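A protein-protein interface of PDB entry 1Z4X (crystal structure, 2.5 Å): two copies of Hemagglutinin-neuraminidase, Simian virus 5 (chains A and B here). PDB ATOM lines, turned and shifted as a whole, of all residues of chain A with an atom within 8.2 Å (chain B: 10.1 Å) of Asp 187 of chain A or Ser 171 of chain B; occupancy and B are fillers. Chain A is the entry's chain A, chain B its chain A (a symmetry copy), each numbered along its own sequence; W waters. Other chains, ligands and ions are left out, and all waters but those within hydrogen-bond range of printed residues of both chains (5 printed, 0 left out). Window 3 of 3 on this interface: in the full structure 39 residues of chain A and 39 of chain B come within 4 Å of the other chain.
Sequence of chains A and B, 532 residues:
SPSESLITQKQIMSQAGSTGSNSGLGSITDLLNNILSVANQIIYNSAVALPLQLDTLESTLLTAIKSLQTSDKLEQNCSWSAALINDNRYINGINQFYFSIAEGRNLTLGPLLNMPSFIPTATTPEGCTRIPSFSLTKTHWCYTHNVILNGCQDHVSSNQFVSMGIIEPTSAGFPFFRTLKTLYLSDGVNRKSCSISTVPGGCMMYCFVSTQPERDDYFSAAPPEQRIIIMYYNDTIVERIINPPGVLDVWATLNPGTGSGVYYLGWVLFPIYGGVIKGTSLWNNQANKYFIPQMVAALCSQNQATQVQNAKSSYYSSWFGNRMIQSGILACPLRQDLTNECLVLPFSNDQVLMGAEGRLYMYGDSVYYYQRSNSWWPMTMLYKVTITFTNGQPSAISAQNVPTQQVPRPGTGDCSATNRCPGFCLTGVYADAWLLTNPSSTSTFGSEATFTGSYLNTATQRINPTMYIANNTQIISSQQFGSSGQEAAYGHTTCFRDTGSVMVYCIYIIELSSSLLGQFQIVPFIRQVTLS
Water W4 bridges the backbone carbonyl oxygen of Asn 114 of chain B (2.7 Å) and the side-chain hydroxyl of Tyr 184 of chain A (2.7 Å).
Water W3 bridges the side-chain carboxylate (OE2) of Glu 168 of chain B and the backbone carbonyl oxygen (O) of Tyr 184 of chain A.
Water W1 bridges OE2 of Glu 168 of chain B and N of Tyr 184 of chain A.
Water W5 lies within hydrogen-bond range of the side-chain hydroxyl (OG) of Ser 171 of chain B, the side-chain amide oxygen (OD1) of Asn 159 of chain A, the backbone NH (N) of Gly 188 of chain A, the side-chain hydroxyl (OG) of Ser 157 of chain A and the backbone carbonyl oxygen (O) of Ser 158 of chain A.
Water W2 lies within hydrogen-bond range of the side-chain amide nitrogen of Asn 159 of chain A, the side-chain hydroxyl of Ser 171 of chain B, the backbone NH of Ala 172 of chain B and the side-chain hydroxyl of Ser 186 of chain A.
Of chain B, only Ser 171 (3.9 Å) comes within 4 Å of Asp 187 of chain A.
No residue of chain B comes within 4 Å of Gly 188 of chain A.
No residue of chain B comes within 4 Å of Val 189 of chain A.
Of the printed residues of chain A, Asn 114 of chain B touches Leu 149 (3.4 Å).
Printed residues of chain A within 4 Å of Pro 116 of chain B: Tyr 184.
Ser 171 of chain B touches three residues of chain A.
The nearest residue of chain B that does not touch Asp 187 of chain A is Thr 170 of chain B (6.2 Å).
The nearest printed residue of chain A that does not touch Phe 174 of chain B is Tyr 184 of chain A (6.3 Å).
No position is printed for both chains.
Of the 9 pairs that touch across the chains among the printed residues, none has its exchanged pair printed and touching as well.
Printed residues of chain B that touch a printed residue of chain A: Asn 114, Pro 116, Thr 170, Ser 171, Phe 174 and Phe 176.
Hydrophobic or aromatic side chains of chain B within 4 Å of the printed part of chain A: Pro 116, Phe 174 and Phe 176.
Among the printed residues, 9 pairs touch across the chains.
Among the printed residues, no Asp or Glu carboxylate lies within 4 Å of a Lys or Arg side-chain nitrogen of the other chain.
Leu 149 of chain A touches Asn 114 of chain B (CD2 to O, 3.4 Å).
Leu 149 of chain A touches Phe 174 of chain B.
Asn 159 of chain A touches Ser 171 of chain B.
CG of Pro 116 of chain B touches CE1 of Tyr 184 of chain A, 3.5 Å away.
Tyr 184 of chain A touches Thr 170 of chain B.
Tyr 184 of chain A touches Phe 176 of chain B (CB to CE2, 3.2 Å).
Thr 170 of chain B touches Ser 186 of chain A.
Ser 171 of chain B touches Asp 187 of chain A (CB to N, 3.9 Å).
The side-chain amide nitrogen (ND2) of Asn 159 of chain A is in hydrogen-bond range of the side-chain hydroxyl (OH) of Tyr 184 of chain A, at 3.1 Å.
The side-chain amide oxygen of Asn 159 of chain A sits at hydrogen-bond distance from the side-chain hydroxyl of Ser 186 of chain A (2.8 Å).
OD1 of Asp 187 of chain A is in hydrogen-bond range of N of Val 189 of chain A (3.0 Å).
The backbone NH (N) of Phe 176 of chain B lies within hydrogen-bond range of the backbone carbonyl oxygen (O) of Glu 168 of chain B, at 2.9 Å.
The side-chain hydroxyl (OG1) of Thr 170 of chain B sits close to the backbone NH (N) of Ala 172 of chain B (3.4 Å).
OG1 of Thr 170 of chain B sits at hydrogen-bond distance from O of Phe 174 of chain B (2.8 Å).
The backbone NH (N) of Ser 171 of chain B is in hydrogen-bond range of the side-chain hydroxyl (OG) of Ser 186 of chain A, at 3.0 Å.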
ATOM      1  N   LEU A 149      20.980 -18.115   2.681  1.00  0.00           N
ATOM      2  CA  LEU A 149      22.049 -17.556   1.858  1.00  0.00           C
ATOM      3  C   LEU A 149      23.053 -16.629   2.552  1.00  0.00           C
ATOM      4  O   LEU A 149      24.254 -16.725   2.304  1.00  0.00           O
ATOM      5  CB  LEU A 149      21.445 -16.857   0.638  1.00  0.00           C
ATOM      6  CG  LEU A 149      20.553 -17.749  -0.241  1.00  0.00           C
ATOM      7  CD1 LEU A 149      20.145 -16.974  -1.497  1.00  0.00           C
ATOM      8  CD2 LEU A 149      21.292 -19.043  -0.614  1.00  0.00           C
ATOM      9  N   VAL A 156      12.197 -14.850   6.653  1.00  0.00           N
ATOM     10  CA  VAL A 156      11.545 -14.588   5.387  1.00  0.00           C
ATOM     11  C   VAL A 156      11.887 -15.586   4.311  1.00  0.00           C
ATOM     12  O   VAL A 156      11.001 -16.167   3.677  1.00  0.00           O
ATOM     13  CB  VAL A 156      11.942 -13.183   4.920  1.00  0.00           C
ATOM     14  CG1 VAL A 156      11.357 -12.886   3.556  1.00  0.00           C
ATOM     15  CG2 VAL A 156      11.483 -12.166   5.947  1.00  0.00           C
ATOM     16  N   SER A 157      13.181 -15.756   4.081  1.00  0.00           N
ATOM     17  CA  SER A 157      13.611 -16.693   3.071  1.00  0.00           C
ATOM     18  C   SER A 157      14.635 -17.652   3.609  1.00  0.00           C
ATOM     19  O   SER A 157      15.436 -17.342   4.487  1.00  0.00           O
ATOM     20  CB  SER A 157      14.198 -15.968   1.855  1.00  0.00           C
ATOM     21  OG  SER A 157      14.567 -16.921   0.852  1.00  0.00           O
ATOM     22  N   SER A 158      14.560 -18.839   3.043  1.00  0.00           N
ATOM     23  CA  SER A 158      15.455 -19.921   3.360  1.00  0.00           C
ATOM     24  C   SER A 158      14.990 -21.064   2.491  1.00  0.00           C
ATOM     25  O   SER A 158      13.867 -21.073   1.988  1.00  0.00           O
ATOM     26  CB  SER A 158      15.359 -20.313   4.836  1.00  0.00           C
ATOM     27  OG  SER A 158      14.244 -21.146   5.077  1.00  0.00           O
ATOM     28  N   ASN A 159      15.878 -22.018   2.295  1.00  0.00           N
ATOM     29  CA  ASN A 159      15.569 -23.183   1.494  1.00  0.00           C
ATOM     30  C   ASN A 159      15.830 -24.390   2.371  1.00  0.00           C
ATOM     31  O   ASN A 159      16.525 -24.286   3.380  1.00  0.00           O
ATOM     32  CB  ASN A 159      16.448 -23.209   0.246  1.00  0.00           C
ATOM     33  CG  ASN A 159      16.222 -22.000  -0.639  1.00  0.00           C
ATOM     34  OD1 ASN A 159      15.087 -21.585  -0.846  1.00  0.00           O
ATOM     35  ND2 ASN A 159      17.302 -21.439  -1.180  1.00  0.00           N
ATOM     36  N   GLN A 160      15.273 -25.530   1.997  1.00  0.00           N
ATOM     37  CA  GLN A 160      15.458 -26.741   2.780  1.00  0.00           C
ATOM     38  C   GLN A 160      15.986 -27.861   1.885  1.00  0.00           C
ATOM     39  O   GLN A 160      15.326 -28.256   0.931  1.00  0.00           O
ATOM     40  CB  GLN A 160      14.124 -27.139   3.404  1.00  0.00           C
ATOM     41  CG  GLN A 160      14.176 -28.251   4.448  1.00  0.00           C
ATOM     42  CD  GLN A 160      14.797 -27.807   5.763  1.00  0.00           C
ATOM     43  OE1 GLN A 160      14.741 -26.630   6.126  1.00  0.00           O
ATOM     44  NE2 GLN A 160      15.373 -28.750   6.493  1.00  0.00           N
ATOM     45  N   TYR A 184      15.828 -29.957  -3.313  1.00  0.00           N
ATOM     46  CA  TYR A 184      16.095 -28.652  -2.726  1.00  0.00           C
ATOM     47  C   TYR A 184      14.806 -27.856  -2.808  1.00  0.00           C
ATOM     48  O   TYR A 184      14.445 -27.346  -3.873  1.00  0.00           O
ATOM     49  CB  TYR A 184      17.223 -27.948  -3.486  1.00  0.00           C
ATOM     50  CG  TYR A 184      17.812 -26.730  -2.795  1.00  0.00           C
ATOM     51  CD1 TYR A 184      18.116 -26.747  -1.427  1.00  0.00           C
ATOM     52  CD2 TYR A 184      18.134 -25.583  -3.524  1.00  0.00           C
ATOM     53  CE1 TYR A 184      18.731 -25.657  -0.807  1.00  0.00           C
ATOM     54  CE2 TYR A 184      18.750 -24.484  -2.918  1.00  0.00           C
ATOM     55  CZ  TYR A 184      19.048 -24.527  -1.560  1.00  0.00           C
ATOM     56  OH  TYR A 184      19.678 -23.446  -0.974  1.00  0.00           O
ATOM     57  N   LEU A 185      14.101 -27.779  -1.685  1.00  0.00           N
ATOM     58  CA  LEU A 185      12.852 -27.046  -1.617  1.00  0.00           C
ATOM     59  C   LEU A 185      13.196 -25.558  -1.555  1.00  0.00           C
ATOM     60  O   LEU A 185      13.574 -25.027  -0.504  1.00  0.00           O
ATOM     61  CB  LEU A 185      12.060 -27.483  -0.383  1.00  0.00           C
ATOM     62  CG  LEU A 185      11.842 -29.002  -0.286  1.00  0.00           C
ATOM     63  CD1 LEU A 185      11.008 -29.340   0.950  1.00  0.00           C
ATOM     64  CD2 LEU A 185      11.140 -29.497  -1.548  1.00  0.00           C
ATOM     65  N   SER A 186      13.084 -24.905  -2.703  1.00  0.00           N
ATOM     66  CA  SER A 186      13.393 -23.491  -2.825  1.00  0.00           C
ATOM     67  C   SER A 186      12.253 -22.862  -3.618  1.00  0.00           C
ATOM     68  O   SER A 186      12.224 -22.961  -4.840  1.00  0.00           O
ATOM     69  CB  SER A 186      14.719 -23.333  -3.569  1.00  0.00           C
ATOM     70  OG  SER A 186      15.130 -21.984  -3.615  1.00  0.00           O
ATOM     71  N   ASP A 187      11.315 -22.222  -2.927  1.00  0.00           N
ATOM     72  CA  ASP A 187      10.166 -21.631  -3.607  1.00  0.00           C
ATOM     73  C   ASP A 187       9.527 -20.455  -2.874  1.00  0.00           C
ATOM     74  O   ASP A 187       8.398 -20.064  -3.193  1.00  0.00           O
ATOM     75  CB  ASP A 187       9.105 -22.709  -3.829  1.00  0.00           C
ATOM     76  CG  ASP A 187       8.566 -23.269  -2.522  1.00  0.00           C
ATOM     77  OD1 ASP A 187       9.013 -22.806  -1.454  1.00  0.00           O
ATOM     78  OD2 ASP A 187       7.700 -24.165  -2.560  1.00  0.00           O
ATOM     79  N   GLY A 188      10.222 -19.898  -1.891  1.00  0.00           N
ATOM     80  CA  GLY A 188       9.662 -18.768  -1.170  1.00  0.00           C
ATOM     81  C   GLY A 188       8.930 -19.106   0.119  1.00  0.00           C
ATOM     82  O   GLY A 188       8.604 -18.210   0.896  1.00  0.00           O
ATOM     83  N   VAL A 189       8.640 -20.382   0.351  1.00  0.00           N
ATOM     84  CA  VAL A 189       7.976 -20.764   1.590  1.00  0.00           C
ATOM     85  C   VAL A 189       9.072 -20.978   2.625  1.00  0.00           C
ATOM     86  O   VAL A 189       9.925 -21.849   2.467  1.00  0.00           O
ATOM     87  CB  VAL A 189       7.153 -22.047   1.417  1.00  0.00           C
ATOM     88  CG1 VAL A 189       6.570 -22.478   2.754  1.00  0.00           C
ATOM     89  CG2 VAL A 189       6.033 -21.798   0.422  1.00  0.00           C
ATOM     90  N   ASN A 190       9.055 -20.175   3.682  1.00  0.00           N
ATOM     91  CA  ASN A 190      10.083 -20.265   4.709  1.00  0.00           C
ATOM     92  C   ASN A 190       9.854 -21.412   5.699  1.00  0.00           C
ATOM     93  O   ASN A 190       9.410 -21.206   6.835  1.00  0.00           O
ATOM     94  CB  ASN A 190      10.191 -18.922   5.437  1.00  0.00           C
ATOM     95  CG  ASN A 190      11.531 -18.734   6.109  1.00  0.00           C
ATOM     96  OD1 ASN A 190      12.536 -19.293   5.674  1.00  0.00           O
ATOM     97  ND2 ASN A 190      11.561 -17.926   7.157  1.00  0.00           N
ATOM     98  N   ARG A 191      10.163 -22.622   5.241  1.00  0.00           N
ATOM     99  CA  ARG A 191      10.023 -23.841   6.034  1.00  0.00           C
ATOM    100  C   ARG A 191      11.159 -23.940   7.046  1.00  0.00           C
ATOM    101  O   ARG A 191      12.331 -23.981   6.672  1.00  0.00           O
ATOM    102  CB  ARG A 191      10.016 -25.065   5.103  1.00  0.00           C
ATOM    103  CG  ARG A 191       8.649 -25.333   4.467  1.00  0.00           C
ATOM    104  CD  ARG A 191       8.706 -26.361   3.347  1.00  0.00           C
ATOM    105  NE  ARG A 191       9.331 -25.760   2.184  1.00  0.00           N
ATOM    106  CZ  ARG A 191       8.724 -25.533   1.023  1.00  0.00           C
ATOM    107  NH1 ARG A 191       7.458 -25.867   0.831  1.00  0.00           N
ATOM    108  NH2 ARG A 191       9.398 -24.926   0.063  1.00  0.00           N
ATOM    109  N   ARG A 227       3.098 -27.574   7.910  1.00  0.00           N
ATOM    110  CA  ARG A 227       3.136 -28.346   6.672  1.00  0.00           C
ATOM    111  C   ARG A 227       3.851 -29.680   6.776  1.00  0.00           C
ATOM    112  O   ARG A 227       4.862 -29.808   7.464  1.00  0.00           O
ATOM    113  CB  ARG A 227       3.809 -27.546   5.565  1.00  0.00           C
ATOM    114  CG  ARG A 227       3.127 -26.249   5.210  1.00  0.00           C
ATOM    115  CD  ARG A 227       3.779 -25.633   3.989  1.00  0.00           C
ATOM    116  NE  ARG A 227       3.042 -24.470   3.505  1.00  0.00           N
ATOM    117  CZ  ARG A 227       2.910 -24.166   2.219  1.00  0.00           C
ATOM    118  NH1 ARG A 227       3.468 -24.940   1.301  1.00  0.00           N
ATOM    119  NH2 ARG A 227       2.213 -23.095   1.850  1.00  0.00           N
ATOM    120  N   GLU A 239       2.841 -32.000  -0.829  1.00  0.00           N
ATOM    121  CA  GLU A 239       2.924 -31.149   0.344  1.00  0.00           C
ATOM    122  C   GLU A 239       1.516 -30.750   0.762  1.00  0.00           C
ATOM    123  O   GLU A 239       0.675 -30.437  -0.079  1.00  0.00           O
ATOM    124  CB  GLU A 239       3.766 -29.900   0.063  1.00  0.00           C
ATOM    125  CG  GLU A 239       3.765 -28.917   1.229  1.00  0.00           C
ATOM    126  CD  GLU A 239       4.902 -27.912   1.168  1.00  0.00           C
ATOM    127  OE1 GLU A 239       5.127 -27.322   0.090  1.00  0.00           O
ATOM    128  OE2 GLU A 239       5.565 -27.703   2.207  1.00  0.00           O
ATOM    129  N   ARG B  89      15.675 -24.325 -18.527  1.00  0.00           N
ATOM    130  CA  ARG B  89      16.462 -23.114 -18.438  1.00  0.00           C
ATOM    131  C   ARG B  89      17.931 -23.293 -18.797  1.00  0.00           C
ATOM    132  O   ARG B  89      18.650 -22.309 -18.968  1.00  0.00           O
ATOM    133  CB  ARG B  89      16.364 -22.550 -17.033  1.00  0.00           C
ATOM    134  CG  ARG B  89      15.078 -21.819 -16.785  1.00  0.00           C
ATOM    135  CD  ARG B  89      15.403 -20.483 -16.180  1.00  0.00           C
ATOM    136  NE  ARG B  89      14.625 -20.279 -14.976  1.00  0.00           N
ATOM    137  CZ  ARG B  89      14.997 -19.503 -13.973  1.00  0.00           C
ATOM    138  NH1 ARG B  89      16.150 -18.848 -14.023  1.00  0.00           N
ATOM    139  NH2 ARG B  89      14.208 -19.393 -12.914  1.00  0.00           N
ATOM    140  N   TYR B  90      18.374 -24.538 -18.922  1.00  0.00           N
ATOM    141  CA  TYR B  90      19.778 -24.778 -19.224  1.00  0.00           C
ATOM    142  C   TYR B  90      20.051 -25.673 -20.425  1.00  0.00           C
ATOM    143  O   TYR B  90      21.154 -25.641 -20.974  1.00  0.00           O
ATOM    144  CB  TYR B  90      20.469 -25.395 -18.006  1.00  0.00           C
ATOM    145  CG  TYR B  90      20.199 -24.673 -16.714  1.00  0.00           C
ATOM    146  CD1 TYR B  90      20.669 -23.381 -16.503  1.00  0.00           C
ATOM    147  CD2 TYR B  90      19.463 -25.282 -15.697  1.00  0.00           C
ATOM    148  CE1 TYR B  90      20.415 -22.709 -15.307  1.00  0.00           C
ATOM    149  CE2 TYR B  90      19.202 -24.617 -14.495  1.00  0.00           C
ATOM    150  CZ  TYR B  90      19.680 -23.334 -14.310  1.00  0.00           C
ATOM    151  OH  TYR B  90      19.420 -22.668 -13.138  1.00  0.00           O
ATOM    152  N   ASN B 114      25.773 -18.828  -2.944  1.00  0.00           N
ATOM    153  CA  ASN B 114      25.702 -20.012  -2.103  1.00  0.00           C
ATOM    154  C   ASN B 114      24.675 -21.045  -2.519  1.00  0.00           C
ATOM    155  O   ASN B 114      23.474 -20.789  -2.495  1.00  0.00           O
ATOM    156  CB  ASN B 114      25.432 -19.636  -0.648  1.00  0.00           C
ATOM    157  CG  ASN B 114      25.447 -20.849   0.267  1.00  0.00           C
ATOM    158  OD1 ASN B 114      26.482 -21.481   0.458  1.00  0.00           O
ATOM    159  ND2 ASN B 114      24.295 -21.185   0.823  1.00  0.00           N
ATOM    160  N   PRO B 116      23.924 -25.575  -2.359  1.00  0.00           N
ATOM    161  CA  PRO B 116      24.370 -26.777  -1.647  1.00  0.00           C
ATOM    162  C   PRO B 116      25.414 -27.489  -2.503  1.00  0.00           C
ATOM    163  O   PRO B 116      25.153 -27.833  -3.656  1.00  0.00           O
ATOM    164  CB  PRO B 116      23.085 -27.592  -1.507  1.00  0.00           C
ATOM    165  CG  PRO B 116      22.006 -26.541  -1.517  1.00  0.00           C
ATOM    166  CD  PRO B 116      22.476 -25.620  -2.608  1.00  0.00           C
ATOM    167  N   GLU B 168      19.001 -27.276 -11.942  1.00  0.00           N
ATOM    168  CA  GLU B 168      17.677 -26.681 -11.873  1.00  0.00           C
ATOM    169  C   GLU B 168      17.770 -25.351 -11.142  1.00  0.00           C
ATOM    170  O   GLU B 168      18.605 -25.172 -10.261  1.00  0.00           O
ATOM    171  CB  GLU B 168      16.691 -27.606 -11.156  1.00  0.00           C
ATOM    172  CG  GLU B 168      17.003 -27.869  -9.697  1.00  0.00           C
ATOM    173  CD  GLU B 168      15.946 -28.738  -9.034  1.00  0.00           C
ATOM    174  OE1 GLU B 168      15.383 -29.617  -9.726  1.00  0.00           O
ATOM    175  OE2 GLU B 168      15.685 -28.556  -7.821  1.00  0.00           O
ATOM    176  N   PRO B 169      16.901 -24.398 -11.499  1.00  0.00           N
ATOM    177  CA  PRO B 169      16.889 -23.070 -10.875  1.00  0.00           C
ATOM    178  C   PRO B 169      16.331 -23.032  -9.457  1.00  0.00           C
ATOM    179  O   PRO B 169      15.431 -23.795  -9.115  1.00  0.00           O
ATOM    180  CB  PRO B 169      16.040 -22.255 -11.842  1.00  0.00           C
ATOM    181  CG  PRO B 169      15.018 -23.263 -12.283  1.00  0.00           C
ATOM    182  CD  PRO B 169      15.857 -24.503 -12.538  1.00  0.00           C
ATOM    183  N   THR B 170      16.884 -22.146  -8.633  1.00  0.00           N
ATOM    184  CA  THR B 170      16.418 -21.971  -7.261  1.00  0.00           C
ATOM    185  C   THR B 170      15.552 -20.719  -7.251  1.00  0.00           C
ATOM    186  O   THR B 170      15.543 -19.965  -8.222  1.00  0.00           O
ATOM    187  CB  THR B 170      17.585 -21.768  -6.275  1.00  0.00           C
ATOM    188  OG1 THR B 170      18.304 -20.577  -6.618  1.00  0.00           O
ATOM    189  CG2 THR B 170      18.529 -22.947  -6.319  1.00  0.00           C
ATOM    190  N   SER B 171      14.832 -20.484  -6.162  1.00  0.00           N
ATOM    191  CA  SER B 171      13.969 -19.310  -6.091  1.00  0.00           C
ATOM    192  C   SER B 171      14.746 -17.997  -6.205  1.00  0.00           C
ATOM    193  O   SER B 171      14.164 -16.955  -6.493  1.00  0.00           O
ATOM    194  CB  SER B 171      13.158 -19.322  -4.794  1.00  0.00           C
ATOM    195  OG  SER B 171      13.988 -19.175  -3.661  1.00  0.00           O
ATOM    196  N   ALA B 172      16.057 -18.049  -5.978  1.00  0.00           N
ATOM    197  CA  ALA B 172      16.889 -16.853  -6.066  1.00  0.00           C
ATOM    198  C   ALA B 172      17.342 -16.636  -7.499  1.00  0.00           C
ATOM    199  O   ALA B 172      17.959 -15.622  -7.827  1.00  0.00           O
ATOM    200  CB  ALA B 172      18.102 -16.980  -5.159  1.00  0.00           C
ATOM    201  N   GLY B 173      17.034 -17.601  -8.354  1.00  0.00           N
ATOM    202  CA  GLY B 173      17.398 -17.485  -9.750  1.00  0.00           C
ATOM    203  C   GLY B 173      18.627 -18.264 -10.170  1.00  0.00           C
ATOM    204  O   GLY B 173      18.735 -18.641 -11.333  1.00  0.00           O
ATOM    205  N   PHE B 174      19.564 -18.512  -9.259  1.00  0.00           N
ATOM    206  CA  PHE B 174      20.748 -19.249  -9.668  1.00  0.00           C
ATOM    207  C   PHE B 174      20.627 -20.766  -9.552  1.00  0.00           C
ATOM    208  O   PHE B 174      19.729 -21.281  -8.890  1.00  0.00           O
ATOM    209  CB  PHE B 174      22.011 -18.701  -8.978  1.00  0.00           C
ATOM    210  CG  PHE B 174      21.945 -18.653  -7.487  1.00  0.00           C
ATOM    211  CD1 PHE B 174      22.236 -19.788  -6.727  1.00  0.00           C
ATOM    212  CD2 PHE B 174      21.673 -17.455  -6.833  1.00  0.00           C
ATOM    213  CE1 PHE B 174      22.270 -19.724  -5.329  1.00  0.00           C
ATOM    214  CE2 PHE B 174      21.700 -17.379  -5.439  1.00  0.00           C
ATOM    215  CZ  PHE B 174      22.001 -18.513  -4.686  1.00  0.00           C
ATOM    216  N   PRO B 175      21.523 -21.497 -10.228  1.00  0.00           N
ATOM    217  CA  PRO B 175      21.561 -22.959 -10.260  1.00  0.00           C
ATOM    218  C   PRO B 175      21.764 -23.739  -8.975  1.00  0.00           C
ATOM    219  O   PRO B 175      22.365 -23.271  -8.015  1.00  0.00           O
ATOM    220  CB  PRO B 175      22.694 -23.264 -11.247  1.00  0.00           C
ATOM    221  CG  PRO B 175      22.800 -22.032 -12.070  1.00  0.00           C
ATOM    222  CD  PRO B 175      22.620 -20.950 -11.046  1.00  0.00           C
ATOM    223  N   PHE B 176      21.245 -24.957  -9.008  1.00  0.00           N
ATOM    224  CA  PHE B 176      21.378 -25.913  -7.936  1.00  0.00           C
ATOM    225  C   PHE B 176      21.700 -27.203  -8.665  1.00  0.00           C
ATOM    226  O   PHE B 176      20.910 -27.664  -9.483  1.00  0.00           O
ATOM    227  CB  PHE B 176      20.072 -26.092  -7.162  1.00  0.00           C
ATOM    228  CG  PHE B 176      19.992 -27.402  -6.408  1.00  0.00           C
ATOM    229  CD1 PHE B 176      21.026 -27.798  -5.558  1.00  0.00           C
ATOM    230  CD2 PHE B 176      18.887 -28.237  -6.547  1.00  0.00           C
ATOM    231  CE1 PHE B 176      20.964 -29.003  -4.857  1.00  0.00           C
ATOM    232  CE2 PHE B 176      18.810 -29.448  -5.848  1.00  0.00           C
ATOM    233  CZ  PHE B 176      19.851 -29.830  -5.003  1.00  0.00           C
ATOM    234  N   ASP B 498      21.939 -19.459 -18.449  1.00  0.00           N
ATOM    235  CA  ASP B 498      20.545 -19.627 -18.105  1.00  0.00           C
ATOM    236  C   ASP B 498      19.870 -18.878 -19.256  1.00  0.00           C
ATOM    237  O   ASP B 498      19.999 -17.656 -19.368  1.00  0.00           O
ATOM    238  CB  ASP B 498      20.243 -18.954 -16.766  1.00  0.00           C
ATOM    239  CG  ASP B 498      18.828 -19.219 -16.278  1.00  0.00           C
ATOM    240  OD1 ASP B 498      17.931 -19.406 -17.132  1.00  0.00           O
ATOM    241  OD2 ASP B 498      18.617 -19.225 -15.047  1.00  0.00           O
ATOM    242  N   TYR B 505      26.674 -18.463 -15.873  1.00  0.00           N
ATOM    243  CA  TYR B 505      27.201 -18.868 -14.586  1.00  0.00           C
ATOM    244  C   TYR B 505      28.397 -19.744 -14.856  1.00  0.00           C
ATOM    245  O   TYR B 505      28.445 -20.467 -15.853  1.00  0.00           O
ATOM    246  CB  TYR B 505      26.175 -19.667 -13.786  1.00  0.00           C
ATOM    247  CG  TYR B 505      25.006 -18.857 -13.288  1.00  0.00           C
ATOM    248  CD1 TYR B 505      23.855 -18.711 -14.062  1.00  0.00           C
ATOM    249  CD2 TYR B 505      25.056 -18.223 -12.049  1.00  0.00           C
ATOM    250  CE1 TYR B 505      22.783 -17.952 -13.613  1.00  0.00           C
ATOM    251  CE2 TYR B 505      23.988 -17.458 -11.591  1.00  0.00           C
ATOM    252  CZ  TYR B 505      22.857 -17.327 -12.380  1.00  0.00           C
ATOM    253  OH  TYR B 505      21.800 -16.562 -11.943  1.00  0.00           O
HETATM  254  O   HOH W   1      14.487 -30.357  -6.151  1.00  0.00           O
HETATM  255  O   HOH W   2      17.071 -19.177  -2.847  1.00  0.00           O
HETATM  256  O   HOH W   3      14.918 -26.345  -6.433  1.00  0.00           O
HETATM  257  O   HOH W   4      20.995 -21.820  -2.718  1.00  0.00           O
HETATM  258  O   HOH W   5      13.256 -19.432  -1.035  1.00  0.00           O
